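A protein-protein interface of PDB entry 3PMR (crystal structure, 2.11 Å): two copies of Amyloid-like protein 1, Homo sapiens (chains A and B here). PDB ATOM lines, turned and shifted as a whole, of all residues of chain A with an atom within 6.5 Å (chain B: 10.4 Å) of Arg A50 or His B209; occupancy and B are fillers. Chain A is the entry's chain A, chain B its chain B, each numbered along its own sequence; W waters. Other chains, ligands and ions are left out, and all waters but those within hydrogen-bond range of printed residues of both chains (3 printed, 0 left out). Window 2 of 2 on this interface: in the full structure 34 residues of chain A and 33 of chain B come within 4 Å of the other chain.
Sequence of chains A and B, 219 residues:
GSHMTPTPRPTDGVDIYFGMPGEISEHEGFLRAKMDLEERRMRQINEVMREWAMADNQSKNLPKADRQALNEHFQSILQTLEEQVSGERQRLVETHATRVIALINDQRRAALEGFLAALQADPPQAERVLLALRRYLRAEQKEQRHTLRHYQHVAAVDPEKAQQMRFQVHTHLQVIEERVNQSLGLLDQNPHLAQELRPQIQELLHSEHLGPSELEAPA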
ATOM      1  N   ARG A  43     -16.409 -11.212 -22.571  1.00  0.00           N
ATOM      2  CA  ARG A  43     -16.113 -11.309 -23.999  1.00  0.00           C
ATOM      3  C   ARG A  43     -15.710  -9.950 -24.567  1.00  0.00           C
ATOM      4  O   ARG A  43     -14.746  -9.848 -25.316  1.00  0.00           O
ATOM      5  CB  ARG A  43     -17.308 -11.856 -24.784  1.00  0.00           C
ATOM      6  CG  ARG A  43     -17.679 -13.290 -24.448  1.00  0.00           C
ATOM      7  CD  ARG A  43     -18.508 -13.903 -25.579  1.00  0.00           C
ATOM      8  NE  ARG A  43     -19.654 -13.066 -25.921  1.00  0.00           N
ATOM      9  CZ  ARG A  43     -20.794 -13.031 -25.234  1.00  0.00           C
ATOM     10  NH1 ARG A  43     -20.955 -13.797 -24.162  1.00  0.00           N
ATOM     11  NH2 ARG A  43     -21.768 -12.213 -25.611  1.00  0.00           N
ATOM     12  N   ILE A  45     -14.463  -7.373 -22.985  1.00  0.00           N
ATOM     13  CA  ILE A  45     -13.143  -7.016 -22.464  1.00  0.00           C
ATOM     14  C   ILE A  45     -12.043  -7.770 -23.211  1.00  0.00           C
ATOM     15  O   ILE A  45     -11.026  -7.194 -23.565  1.00  0.00           O
ATOM     16  CB  ILE A  45     -13.017  -7.351 -20.961  1.00  0.00           C
ATOM     17  CG1 ILE A  45     -13.868  -6.384 -20.124  1.00  0.00           C
ATOM     18  CG2 ILE A  45     -11.560  -7.301 -20.538  1.00  0.00           C
ATOM     19  CD1 ILE A  45     -13.832  -6.677 -18.626  1.00  0.00           C
ATOM     20  N   ASN A  46     -12.250  -9.058 -23.445  1.00  0.00           N
ATOM     21  CA  ASN A  46     -11.256  -9.861 -24.145  1.00  0.00           C
ATOM     22  C   ASN A  46     -11.082  -9.347 -25.575  1.00  0.00           C
ATOM     23  O   ASN A  46      -9.967  -9.322 -26.097  1.00  0.00           O
ATOM     24  CB  ASN A  46     -11.666 -11.330 -24.177  1.00  0.00           C
ATOM     25  CG  ASN A  46     -10.509 -12.248 -24.564  1.00  0.00           C
ATOM     26  OD1 ASN A  46      -9.371 -12.022 -24.156  1.00  0.00           O
ATOM     27  ND2 ASN A  46     -10.799 -13.292 -25.328  1.00  0.00           N
ATOM     28  N   GLU A  47     -12.177  -8.938 -26.212  1.00  0.00           N
ATOM     29  CA  GLU A  47     -12.066  -8.425 -27.572  1.00  0.00           C
ATOM     30  C   GLU A  47     -11.154  -7.199 -27.587  1.00  0.00           C
ATOM     31  O   GLU A  47     -10.283  -7.087 -28.442  1.00  0.00           O
ATOM     32  CB  GLU A  47     -13.441  -8.065 -28.139  1.00  0.00           C
ATOM     33  CG  GLU A  47     -13.417  -7.758 -29.630  1.00  0.00           C
ATOM     34  N   VAL A  48     -11.337  -6.283 -26.642  1.00  0.00           N
ATOM     35  CA  VAL A  48     -10.498  -5.088 -26.596  1.00  0.00           C
ATOM     36  C   VAL A  48      -9.041  -5.440 -26.297  1.00  0.00           C
ATOM     37  O   VAL A  48      -8.123  -4.855 -26.883  1.00  0.00           O
ATOM     38  CB  VAL A  48     -10.998  -4.088 -25.525  1.00  0.00           C
ATOM     39  CG1 VAL A  48     -10.022  -2.940 -25.383  1.00  0.00           C
ATOM     40  CG2 VAL A  48     -12.363  -3.542 -25.918  1.00  0.00           C
ATOM     41  N   MET A  49      -8.832  -6.387 -25.380  1.00  0.00           N
ATOM     42  CA  MET A  49      -7.475  -6.804 -25.018  1.00  0.00           C
ATOM     43  C   MET A  49      -6.732  -7.394 -26.229  1.00  0.00           C
ATOM     44  O   MET A  49      -5.554  -7.129 -26.424  1.00  0.00           O
ATOM     45  CB  MET A  49      -7.514  -7.817 -23.858  1.00  0.00           C
ATOM     46  CG  MET A  49      -7.919  -7.244 -22.495  1.00  0.00           C
ATOM     47  SD  MET A  49      -6.802  -5.988 -21.856  1.00  0.00           S
ATOM     48  CE  MET A  49      -7.725  -5.428 -20.353  1.00  0.00           C
ATOM     49  N   ARG A  50      -7.431  -8.179 -27.048  1.00  0.00           N
ATOM     50  CA  ARG A  50      -6.835  -8.786 -28.243  1.00  0.00           C
ATOM     51  C   ARG A  50      -6.425  -7.724 -29.269  1.00  0.00           C
ATOM     52  O   ARG A  50      -5.367  -7.826 -29.889  1.00  0.00           O
ATOM     53  CB  ARG A  50      -7.817  -9.754 -28.906  1.00  0.00           C
ATOM     54  CG  ARG A  50      -8.126 -11.009 -28.114  1.00  0.00           C
ATOM     55  CD  ARG A  50      -9.208 -11.836 -28.809  1.00  0.00           C
ATOM     56  NE  ARG A  50      -8.754 -13.181 -29.160  1.00  0.00           N
ATOM     57  CZ  ARG A  50      -9.390 -13.978 -30.017  1.00  0.00           C
ATOM     58  NH1 ARG A  50     -10.504 -13.561 -30.611  1.00  0.00           N
ATOM     59  NH2 ARG A  50      -8.918 -15.192 -30.282  1.00  0.00           N
ATOM     60  N   GLU A  51      -7.269  -6.714 -29.456  1.00  0.00           N
ATOM     61  CA  GLU A  51      -6.980  -5.631 -30.399  1.00  0.00           C
ATOM     62  C   GLU A  51      -5.771  -4.845 -29.921  1.00  0.00           C
ATOM     63  O   GLU A  51      -4.919  -4.442 -30.707  1.00  0.00           O
ATOM     64  CB  GLU A  51      -8.173  -4.685 -30.512  1.00  0.00           C
ATOM     65  CG  GLU A  51      -9.385  -5.309 -31.140  1.00  0.00           C
ATOM     66  CD  GLU A  51     -10.576  -4.373 -31.141  1.00  0.00           C
ATOM     67  OE1 GLU A  51     -10.825  -3.732 -30.098  1.00  0.00           O
ATOM     68  OE2 GLU A  51     -11.265  -4.280 -32.176  1.00  0.00           O
ATOM     69  N   TRP A  52      -5.706  -4.644 -28.616  1.00  0.00           N
ATOM     70  CA  TRP A  52      -4.602  -3.924 -28.002  1.00  0.00           C
ATOM     71  C   TRP A  52      -3.319  -4.715 -28.191  1.00  0.00           C
ATOM     72  O   TRP A  52      -2.265  -4.157 -28.495  1.00  0.00           O
ATOM     73  CB  TRP A  52      -4.879  -3.753 -26.515  1.00  0.00           C
ATOM     74  CG  TRP A  52      -3.951  -2.846 -25.780  1.00  0.00           C
ATOM     75  CD1 TRP A  52      -2.848  -2.210 -26.274  1.00  0.00           C
ATOM     76  CD2 TRP A  52      -4.036  -2.493 -24.394  1.00  0.00           C
ATOM     77  NE1 TRP A  52      -2.242  -1.484 -25.275  1.00  0.00           N
ATOM     78  CE2 TRP A  52      -2.951  -1.639 -24.112  1.00  0.00           C
ATOM     79  CE3 TRP A  52      -4.935  -2.811 -23.360  1.00  0.00           C
ATOM     80  CZ2 TRP A  52      -2.724  -1.108 -22.832  1.00  0.00           C
ATOM     81  CZ3 TRP A  52      -4.710  -2.281 -22.086  1.00  0.00           C
ATOM     82  CH2 TRP A  52      -3.614  -1.435 -21.836  1.00  0.00           C
ATOM     83  N   ALA A  53      -3.414  -6.022 -27.993  1.00  0.00           N
ATOM     84  CA  ALA A  53      -2.261  -6.894 -28.149  1.00  0.00           C
ATOM     85  C   ALA A  53      -1.848  -6.879 -29.612  1.00  0.00           C
ATOM     86  O   ALA A  53      -0.676  -6.733 -29.938  1.00  0.00           O
ATOM     87  CB  ALA A  53      -2.616  -8.305 -27.712  1.00  0.00           C
ATOM     88  N   MET A  54      -2.828  -7.000 -30.497  1.00  0.00           N
ATOM     89  CA  MET A  54      -2.548  -6.983 -31.925  1.00  0.00           C
ATOM     90  C   MET A  54      -1.957  -5.642 -32.372  1.00  0.00           C
ATOM     91  O   MET A  54      -0.971  -5.606 -33.103  1.00  0.00           O
ATOM     92  CB  MET A  54      -3.821  -7.287 -32.712  1.00  0.00           C
ATOM     93  CG  MET A  54      -3.578  -7.386 -34.193  1.00  0.00           C
ATOM     94  SD  MET A  54      -5.068  -7.159 -35.155  1.00  0.00           S
ATOM     95  CE  MET A  54      -4.469  -7.614 -36.793  1.00  0.00           C
ATOM     96  N   ALA A  55      -2.554  -4.541 -31.926  1.00  0.00           N
ATOM     97  CA  ALA A  55      -2.064  -3.213 -32.290  1.00  0.00           C
ATOM     98  C   ALA A  55      -0.643  -2.990 -31.790  1.00  0.00           C
ATOM     99  O   ALA A  55       0.089  -2.154 -32.311  1.00  0.00           O
ATOM    100  CB  ALA A  55      -2.980  -2.138 -31.732  1.00  0.00           C
ATOM    101  N   LEU B 137      -4.307 -26.342 -23.542  1.00  0.00           N
ATOM    102  CA  LEU B 137      -4.975 -25.143 -24.036  1.00  0.00           C
ATOM    103  C   LEU B 137      -6.198 -24.837 -23.183  1.00  0.00           C
ATOM    104  O   LEU B 137      -6.521 -23.679 -22.942  1.00  0.00           O
ATOM    105  CB  LEU B 137      -5.383 -25.322 -25.505  1.00  0.00           C
ATOM    106  CG  LEU B 137      -4.198 -25.456 -26.463  1.00  0.00           C
ATOM    107  CD1 LEU B 137      -4.666 -25.590 -27.894  1.00  0.00           C
ATOM    108  CD2 LEU B 137      -3.329 -24.224 -26.322  1.00  0.00           C
ATOM    109  N   ARG B 138      -6.884 -25.878 -22.720  1.00  0.00           N
ATOM    110  CA  ARG B 138      -8.049 -25.661 -21.878  1.00  0.00           C
ATOM    111  C   ARG B 138      -7.611 -25.140 -20.512  1.00  0.00           C
ATOM    112  O   ARG B 138      -8.337 -24.384 -19.871  1.00  0.00           O
ATOM    113  CB  ARG B 138      -8.861 -26.948 -21.724  1.00  0.00           C
ATOM    114  CG  ARG B 138      -9.496 -27.396 -23.026  1.00  0.00           C
ATOM    115  CD  ARG B 138     -10.691 -28.305 -22.794  1.00  0.00           C
ATOM    116  NE  ARG B 138     -10.828 -28.695 -21.394  1.00  0.00           N
ATOM    117  N   GLU B 140      -5.127 -23.179 -20.125  1.00  0.00           N
ATOM    118  CA  GLU B 140      -4.830 -21.769 -20.384  1.00  0.00           C
ATOM    119  C   GLU B 140      -6.092 -20.935 -20.577  1.00  0.00           C
ATOM    120  O   GLU B 140      -6.134 -19.772 -20.182  1.00  0.00           O
ATOM    121  CB  GLU B 140      -3.891 -21.621 -21.585  1.00  0.00           C
ATOM    122  CG  GLU B 140      -2.452 -21.887 -21.195  1.00  0.00           C
ATOM    123  CD  GLU B 140      -2.052 -21.115 -19.936  1.00  0.00           C
ATOM    124  OE1 GLU B 140      -1.296 -20.131 -20.050  1.00  0.00           O
ATOM    125  OE2 GLU B 140      -2.507 -21.490 -18.827  1.00  0.00           O
ATOM    126  N   GLN B 141      -7.120 -21.540 -21.164  1.00  0.00           N
ATOM    127  CA  GLN B 141      -8.390 -20.854 -21.348  1.00  0.00           C
ATOM    128  C   GLN B 141      -8.969 -20.569 -19.966  1.00  0.00           C
ATOM    129  O   GLN B 141      -9.496 -19.490 -19.713  1.00  0.00           O
ATOM    130  CB  GLN B 141      -9.371 -21.720 -22.135  1.00  0.00           C
ATOM    131  CG  GLN B 141     -10.739 -21.083 -22.265  1.00  0.00           C
ATOM    132  CD  GLN B 141     -11.782 -22.036 -22.807  1.00  0.00           C
ATOM    133  OE1 GLN B 141     -11.910 -23.172 -22.340  1.00  0.00           O
ATOM    134  NE2 GLN B 141     -12.546 -21.576 -23.790  1.00  0.00           N
ATOM    135  N   LYS B 142      -8.858 -21.541 -19.065  1.00  0.00           N
ATOM    136  CA  LYS B 142      -9.372 -21.358 -17.704  1.00  0.00           C
ATOM    137  C   LYS B 142      -8.664 -20.188 -17.005  1.00  0.00           C
ATOM    138  O   LYS B 142      -9.299 -19.395 -16.319  1.00  0.00           O
ATOM    139  CB  LYS B 142      -9.186 -22.647 -16.899  1.00  0.00           C
ATOM    140  CG  LYS B 142      -9.903 -22.650 -15.570  1.00  0.00           C
ATOM    141  CD  LYS B 142     -10.111 -24.066 -15.059  1.00  0.00           C
ATOM    142  CE  LYS B 142     -11.184 -24.076 -13.993  1.00  0.00           C
ATOM    143  NZ  LYS B 142     -12.401 -23.420 -14.538  1.00  0.00           N
ATOM    144  N   GLN B 144      -7.200 -17.665 -18.484  1.00  0.00           N
ATOM    145  CA  GLN B 144      -7.566 -16.452 -19.184  1.00  0.00           C
ATOM    146  C   GLN B 144      -8.916 -15.963 -18.673  1.00  0.00           C
ATOM    147  O   GLN B 144      -9.081 -14.787 -18.349  1.00  0.00           O
ATOM    148  CB  GLN B 144      -7.653 -16.715 -20.685  1.00  0.00           C
ATOM    149  CG  GLN B 144      -8.099 -15.505 -21.456  1.00  0.00           C
ATOM    150  CD  GLN B 144      -8.163 -15.765 -22.930  1.00  0.00           C
ATOM    151  OE1 GLN B 144      -9.134 -16.332 -23.435  1.00  0.00           O
ATOM    152  NE2 GLN B 144      -7.114 -15.366 -23.640  1.00  0.00           N
ATOM    153  N   ARG B 145      -9.878 -16.874 -18.593  1.00  0.00           N
ATOM    154  CA  ARG B 145     -11.210 -16.525 -18.115  1.00  0.00           C
ATOM    155  C   ARG B 145     -11.149 -16.037 -16.678  1.00  0.00           C
ATOM    156  O   ARG B 145     -11.893 -15.139 -16.285  1.00  0.00           O
ATOM    157  CB  ARG B 145     -12.150 -17.732 -18.235  1.00  0.00           C
ATOM    158  CG  ARG B 145     -12.610 -17.997 -19.676  1.00  0.00           C
ATOM    159  CD  ARG B 145     -13.340 -19.325 -19.814  1.00  0.00           C
ATOM    160  NE  ARG B 145     -14.535 -19.402 -18.978  1.00  0.00           N
ATOM    161  CZ  ARG B 145     -15.636 -18.674 -19.162  1.00  0.00           C
ATOM    162  NH1 ARG B 145     -15.706 -17.801 -20.160  1.00  0.00           N
ATOM    163  NH2 ARG B 145     -16.671 -18.822 -18.345  1.00  0.00           N
ATOM    164  N   LEU B 148      -9.938 -12.432 -16.811  1.00  0.00           N
ATOM    165  CA  LEU B 148     -11.002 -11.579 -17.331  1.00  0.00           C
ATOM    166  C   LEU B 148     -12.137 -11.395 -16.325  1.00  0.00           C
ATOM    167  O   LEU B 148     -12.621 -10.277 -16.126  1.00  0.00           O
ATOM    168  CB  LEU B 148     -11.565 -12.171 -18.633  1.00  0.00           C
ATOM    169  CG  LEU B 148     -10.636 -12.259 -19.856  1.00  0.00           C
ATOM    170  CD1 LEU B 148     -11.184 -13.256 -20.853  1.00  0.00           C
ATOM    171  CD2 LEU B 148     -10.492 -10.887 -20.503  1.00  0.00           C
ATOM    172  N   VAL B 169      -3.790  -6.617 -16.241  1.00  0.00           N
ATOM    173  CA  VAL B 169      -4.659  -7.607 -16.865  1.00  0.00           C
ATOM    174  C   VAL B 169      -4.101  -7.834 -18.275  1.00  0.00           C
ATOM    175  O   VAL B 169      -3.861  -8.961 -18.687  1.00  0.00           O
ATOM    176  CB  VAL B 169      -6.119  -7.095 -16.955  1.00  0.00           C
ATOM    177  CG1 VAL B 169      -6.968  -8.072 -17.752  1.00  0.00           C
ATOM    178  CG2 VAL B 169      -6.697  -6.925 -15.550  1.00  0.00           C
ATOM    179  N   HIS B 170      -3.883  -6.739 -18.993  1.00  0.00           N
ATOM    180  CA  HIS B 170      -3.319  -6.769 -20.341  1.00  0.00           C
ATOM    181  C   HIS B 170      -2.012  -7.575 -20.355  1.00  0.00           C
ATOM    182  O   HIS B 170      -1.806  -8.413 -21.225  1.00  0.00           O
ATOM    183  CB  HIS B 170      -3.050  -5.336 -20.791  1.00  0.00           C
ATOM    184  CG  HIS B 170      -2.298  -5.218 -22.083  1.00  0.00           C
ATOM    185  ND1 HIS B 170      -2.727  -5.798 -23.260  1.00  0.00           N
ATOM    186  CD2 HIS B 170      -1.181  -4.518 -22.395  1.00  0.00           C
ATOM    187  CE1 HIS B 170      -1.910  -5.456 -24.241  1.00  0.00           C
ATOM    188  NE2 HIS B 170      -0.964  -4.680 -23.742  1.00  0.00           N
ATOM    189  N   THR B 171      -1.145  -7.330 -19.377  1.00  0.00           N
ATOM    190  CA  THR B 171       0.140  -8.018 -19.301  1.00  0.00           C
ATOM    191  C   THR B 171      -0.043  -9.529 -19.091  1.00  0.00           C
ATOM    192  O   THR B 171       0.568 -10.343 -19.790  1.00  0.00           O
ATOM    193  CB  THR B 171       1.004  -7.419 -18.165  1.00  0.00           C
ATOM    194  OG1 THR B 171       1.210  -6.022 -18.412  1.00  0.00           O
ATOM    195  CG2 THR B 171       2.359  -8.100 -18.094  1.00  0.00           C
ATOM    196  N   LEU B 173      -2.605 -11.325 -19.819  1.00  0.00           N
ATOM    197  CA  LEU B 173      -3.150 -11.924 -21.033  1.00  0.00           C
ATOM    198  C   LEU B 173      -2.039 -12.144 -22.063  1.00  0.00           C
ATOM    199  O   LEU B 173      -2.081 -13.110 -22.811  1.00  0.00           O
ATOM    200  CB  LEU B 173      -4.270 -11.053 -21.617  1.00  0.00           C
ATOM    201  CG  LEU B 173      -5.550 -11.100 -20.778  1.00  0.00           C
ATOM    202  CD1 LEU B 173      -6.592 -10.174 -21.387  1.00  0.00           C
ATOM    203  CD2 LEU B 173      -6.083 -12.529 -20.725  1.00  0.00           C
ATOM    204  N   GLN B 174      -1.037 -11.270 -22.092  1.00  0.00           N
ATOM    205  CA  GLN B 174       0.077 -11.449 -23.034  1.00  0.00           C
ATOM    206  C   GLN B 174       0.966 -12.622 -22.590  1.00  0.00           C
ATOM    207  O   GLN B 174       1.594 -13.275 -23.420  1.00  0.00           O
ATOM    208  CB  GLN B 174       0.948 -10.192 -23.122  1.00  0.00           C
ATOM    209  CG  GLN B 174       0.247  -8.947 -23.642  1.00  0.00           C
ATOM    210  CD  GLN B 174       1.201  -7.758 -23.747  1.00  0.00           C
ATOM    211  OE1 GLN B 174       2.001  -7.508 -22.845  1.00  0.00           O
ATOM    212  NE2 GLN B 174       1.117  -7.025 -24.849  1.00  0.00           N
ATOM    213  N   ILE B 176      -0.137 -15.337 -21.097  1.00  0.00           N
ATOM    214  CA  ILE B 176      -0.892 -16.523 -21.456  1.00  0.00           C
ATOM    215  C   ILE B 176      -0.764 -16.786 -22.950  1.00  0.00           C
ATOM    216  O   ILE B 176      -0.626 -17.927 -23.385  1.00  0.00           O
ATOM    217  CB  ILE B 176      -2.373 -16.335 -21.131  1.00  0.00           C
ATOM    218  CG1 ILE B 176      -2.561 -16.277 -19.624  1.00  0.00           C
ATOM    219  CG2 ILE B 176      -3.192 -17.445 -21.758  1.00  0.00           C
ATOM    220  CD1 ILE B 176      -3.987 -16.018 -19.231  1.00  0.00           C
ATOM    221  N   GLU B 177      -0.820 -15.713 -23.730  1.00  0.00           N
ATOM    222  CA  GLU B 177      -0.723 -15.816 -25.178  1.00  0.00           C
ATOM    223  C   GLU B 177       0.649 -16.337 -25.568  1.00  0.00           C
ATOM    224  O   GLU B 177       0.787 -17.103 -26.516  1.00  0.00           O
ATOM    225  CB  GLU B 177      -0.962 -14.452 -25.831  1.00  0.00           C
ATOM    226  CG  GLU B 177      -0.896 -14.488 -27.344  1.00  0.00           C
ATOM    227  N   VAL B 180       0.930 -20.131 -24.923  1.00  0.00           N
ATOM    228  CA  VAL B 180       0.255 -20.848 -25.991  1.00  0.00           C
ATOM    229  C   VAL B 180       1.175 -20.928 -27.224  1.00  0.00           C
ATOM    230  O   VAL B 180       1.315 -21.993 -27.832  1.00  0.00           O
ATOM    231  CB  VAL B 180      -1.066 -20.150 -26.384  1.00  0.00           C
ATOM    232  CG1 VAL B 180      -1.690 -20.840 -27.595  1.00  0.00           C
ATOM    233  CG2 VAL B 180      -2.038 -20.168 -25.192  1.00  0.00           C
ATOM    234  N   ILE B 201      -5.903 -27.964 -34.327  1.00  0.00           N
ATOM    235  CA  ILE B 201      -5.415 -26.995 -33.352  1.00  0.00           C
ATOM    236  C   ILE B 201      -6.039 -25.628 -33.591  1.00  0.00           C
ATOM    237  O   ILE B 201      -6.355 -24.905 -32.644  1.00  0.00           O
ATOM    238  CB  ILE B 201      -3.896 -26.838 -33.430  1.00  0.00           C
ATOM    239  CG1 ILE B 201      -3.219 -28.158 -33.054  1.00  0.00           C
ATOM    240  CG2 ILE B 201      -3.447 -25.705 -32.510  1.00  0.00           C
ATOM    241  CD1 ILE B 201      -1.724 -28.166 -33.283  1.00  0.00           C
ATOM    242  N   GLN B 202      -6.192 -25.269 -34.862  1.00  0.00           N
ATOM    243  CA  GLN B 202      -6.795 -23.995 -35.223  1.00  0.00           C
ATOM    244  C   GLN B 202      -8.221 -23.927 -34.699  1.00  0.00           C
ATOM    245  O   GLN B 202      -8.656 -22.891 -34.187  1.00  0.00           O
ATOM    246  CB  GLN B 202      -6.794 -23.818 -36.742  1.00  0.00           C
ATOM    247  CG  GLN B 202      -6.062 -22.558 -37.195  1.00  0.00           C
ATOM    248  CD  GLN B 202      -4.585 -22.566 -36.797  1.00  0.00           C
ATOM    249  OE1 GLN B 202      -3.802 -23.371 -37.307  1.00  0.00           O
ATOM    250  NE2 GLN B 202      -4.199 -21.666 -35.875  1.00  0.00           N
ATOM    251  N   GLU B 203      -8.946 -25.034 -34.833  1.00  0.00           N
ATOM    252  CA  GLU B 203     -10.320 -25.088 -34.358  1.00  0.00           C
ATOM    253  C   GLU B 203     -10.328 -24.895 -32.843  1.00  0.00           C
ATOM    254  O   GLU B 203     -11.191 -24.203 -32.295  1.00  0.00           O
ATOM    255  CB  GLU B 203     -10.971 -26.429 -34.728  1.00  0.00           C
ATOM    256  CG  GLU B 203     -12.445 -26.534 -34.342  1.00  0.00           C
ATOM    257  N   LEU B 204      -9.354 -25.502 -32.168  1.00  0.00           N
ATOM    258  CA  LEU B 204      -9.245 -25.381 -30.718  1.00  0.00           C
ATOM    259  C   LEU B 204      -9.014 -23.921 -30.323  1.00  0.00           C
ATOM    260  O   LEU B 204      -9.755 -23.364 -29.508  1.00  0.00           O
ATOM    261  CB  LEU B 204      -8.084 -26.233 -30.188  1.00  0.00           C
ATOM    262  CG  LEU B 204      -8.135 -27.757 -30.383  1.00  0.00           C
ATOM    263  CD1 LEU B 204      -6.830 -28.371 -29.907  1.00  0.00           C
ATOM    264  CD2 LEU B 204      -9.313 -28.355 -29.620  1.00  0.00           C
ATOM    265  N   LEU B 205      -7.989 -23.307 -30.908  1.00  0.00           N
ATOM    266  CA  LEU B 205      -7.647 -21.913 -30.617  1.00  0.00           C
ATOM    267  C   LEU B 205      -8.790 -20.942 -30.888  1.00  0.00           C
ATOM    268  O   LEU B 205      -8.884 -19.897 -30.244  1.00  0.00           O
ATOM    269  CB  LEU B 205      -6.431 -21.483 -31.438  1.00  0.00           C
ATOM    270  CG  LEU B 205      -5.159 -22.322 -31.283  1.00  0.00           C
ATOM    271  CD1 LEU B 205      -4.122 -21.862 -32.293  1.00  0.00           C
ATOM    272  CD2 LEU B 205      -4.615 -22.205 -29.864  1.00  0.00           C
ATOM    273  N   HIS B 206      -9.650 -21.281 -31.844  1.00  0.00           N
ATOM    274  CA  HIS B 206     -10.779 -20.424 -32.200  1.00  0.00           C
ATOM    275  C   HIS B 206     -11.910 -20.510 -31.185  1.00  0.00           C
ATOM    276  O   HIS B 206     -12.469 -19.495 -30.767  1.00  0.00           O
ATOM    277  CB  HIS B 206     -11.304 -20.800 -33.590  1.00  0.00           C
ATOM    278  N   SER B 207     -12.241 -21.732 -30.785  1.00  0.00           N
ATOM    279  CA  SER B 207     -13.315 -21.952 -29.827  1.00  0.00           C
ATOM    280  C   SER B 207     -12.926 -21.541 -28.410  1.00  0.00           C
ATOM    281  O   SER B 207     -13.772 -21.077 -27.640  1.00  0.00           O
ATOM    282  CB  SER B 207     -13.736 -23.418 -29.850  1.00  0.00           C
ATOM    283  OG  SER B 207     -12.620 -24.268 -29.665  1.00  0.00           O
ATOM    284  N   GLU B 208     -11.648 -21.707 -28.070  1.00  0.00           N
ATOM    285  CA  GLU B 208     -11.167 -21.329 -26.746  1.00  0.00           C
ATOM    286  C   GLU B 208     -11.067 -19.811 -26.631  1.00  0.00           C
ATOM    287  O   GLU B 208     -10.838 -19.281 -25.556  1.00  0.00           O
ATOM    288  CB  GLU B 208      -9.812 -21.986 -26.448  1.00  0.00           C
ATOM    289  CG  GLU B 208      -9.857 -23.507 -26.296  1.00  0.00           C
ATOM    290  N   HIS B 209     -11.227 -19.113 -27.750  1.00  0.00           N
ATOM    291  CA  HIS B 209     -11.188 -17.657 -27.721  1.00  0.00           C
ATOM    292  C   HIS B 209     -12.529 -17.188 -27.180  1.00  0.00           C
ATOM    293  O   HIS B 209     -12.537 -16.222 -26.395  1.00  0.00           O
ATOM    294  CB  HIS B 209     -10.926 -17.075 -29.125  1.00  0.00           C
HETATM  295  O   HOH W   1      -6.812 -12.684 -24.718  1.00  0.00           O
HETATM  296  O   HOH W   2      -3.829  -8.278 -24.235  1.00  0.00           O
HETATM  297  O   HOH W   3      -9.094 -17.688 -31.601  1.00  0.00           O
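The side-chain amide nitrogen (NE2) of Gln B174 lies within hydrogen-bond range of a ring nitrogen (NE2) of His B170, at 3.3 Å.
Among the printed residues, merely in contact across the chains: Arg A50 with His B209 (3.0 Å), Met A49 with Leu B173 (3.4 Å), Asn A46 with His B209 (3.6 Å), Trp A52 with His B170 (3.7 Å), Ile A45 with Leu B148 (3.7 Å), Met A49 with Val B169 (3.8 Å), Asn A46 with Leu B148 (3.9 Å), Met A49 with His B170 (3.9 Å) and Asn A46 with Gln B144 (3.9 Å).
Printed residues of chain B within 4 Å of Ile A45: Leu B148 (3.7 Å).
Of chain B, only Gln B144 (3.9 Å), Leu B148 (3.9 Å) and His B209 (3.6 Å) come within 4 Å of Asn A46.
No residue of chain B comes within 4 Å of Glu A47.
Of the printed residues of chain B, Met A49 touches Val B169 (3.8 Å), His B170 (3.9 Å) and Leu B173 (3.4 Å).
Of chain B, only His B209 comes within 4 Å of Arg A50.
Met A54 touches none of the printed residues of chain B.
Of the printed residues of chain A, Gln B144 touches Asn A46 (3.9 Å).
Printed residues of chain A within 4 Å of Val B169: Met A49 (3.8 Å).
Leu B205 touches none of the printed residues of chain A.
Of chain A, only Asn A46 and Arg A50 come within 4 Å of His B209.
The nearest residue of chain A that does not touch His B209 is Arg A43 (6.2 Å).
The nearest printed residue of chain A that does not touch Val B169 is Ile A45 (5.4 Å).
Hydrophobic or aromatic side chains of chain B within 4 Å of the printed part of chain A: Leu B148, Val B169, His B170, Leu B173 and His B209.
Of the 12 printed residues of chain A, 5 touch a printed residue of chain B.
Among the printed residues, 9 pairs touch across the chains.
Among the printed residues, no Asp or Glu carboxylate lies within 4 Å of a Lys or Arg side-chain nitrogen of the other chain.
No position is printed for both chains.
Of the 9 pairs that touch across the chains among the printed residues, none has its exchanged pair printed and touching as well.
Water W3 lies within hydrogen-bond range of O of Leu B205 (2.6 Å) and NH2 of Arg A50 (2.8 Å).
Water W1 lies within hydrogen-bond range of OD1 of Asn A46 (2.7 Å) and NE2 of Gln B144 (2.9 Å).
Water W2 lies within hydrogen-bond range of ND1 of His B170 (2.9 Å) and O of Met A49 (3.0 Å).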
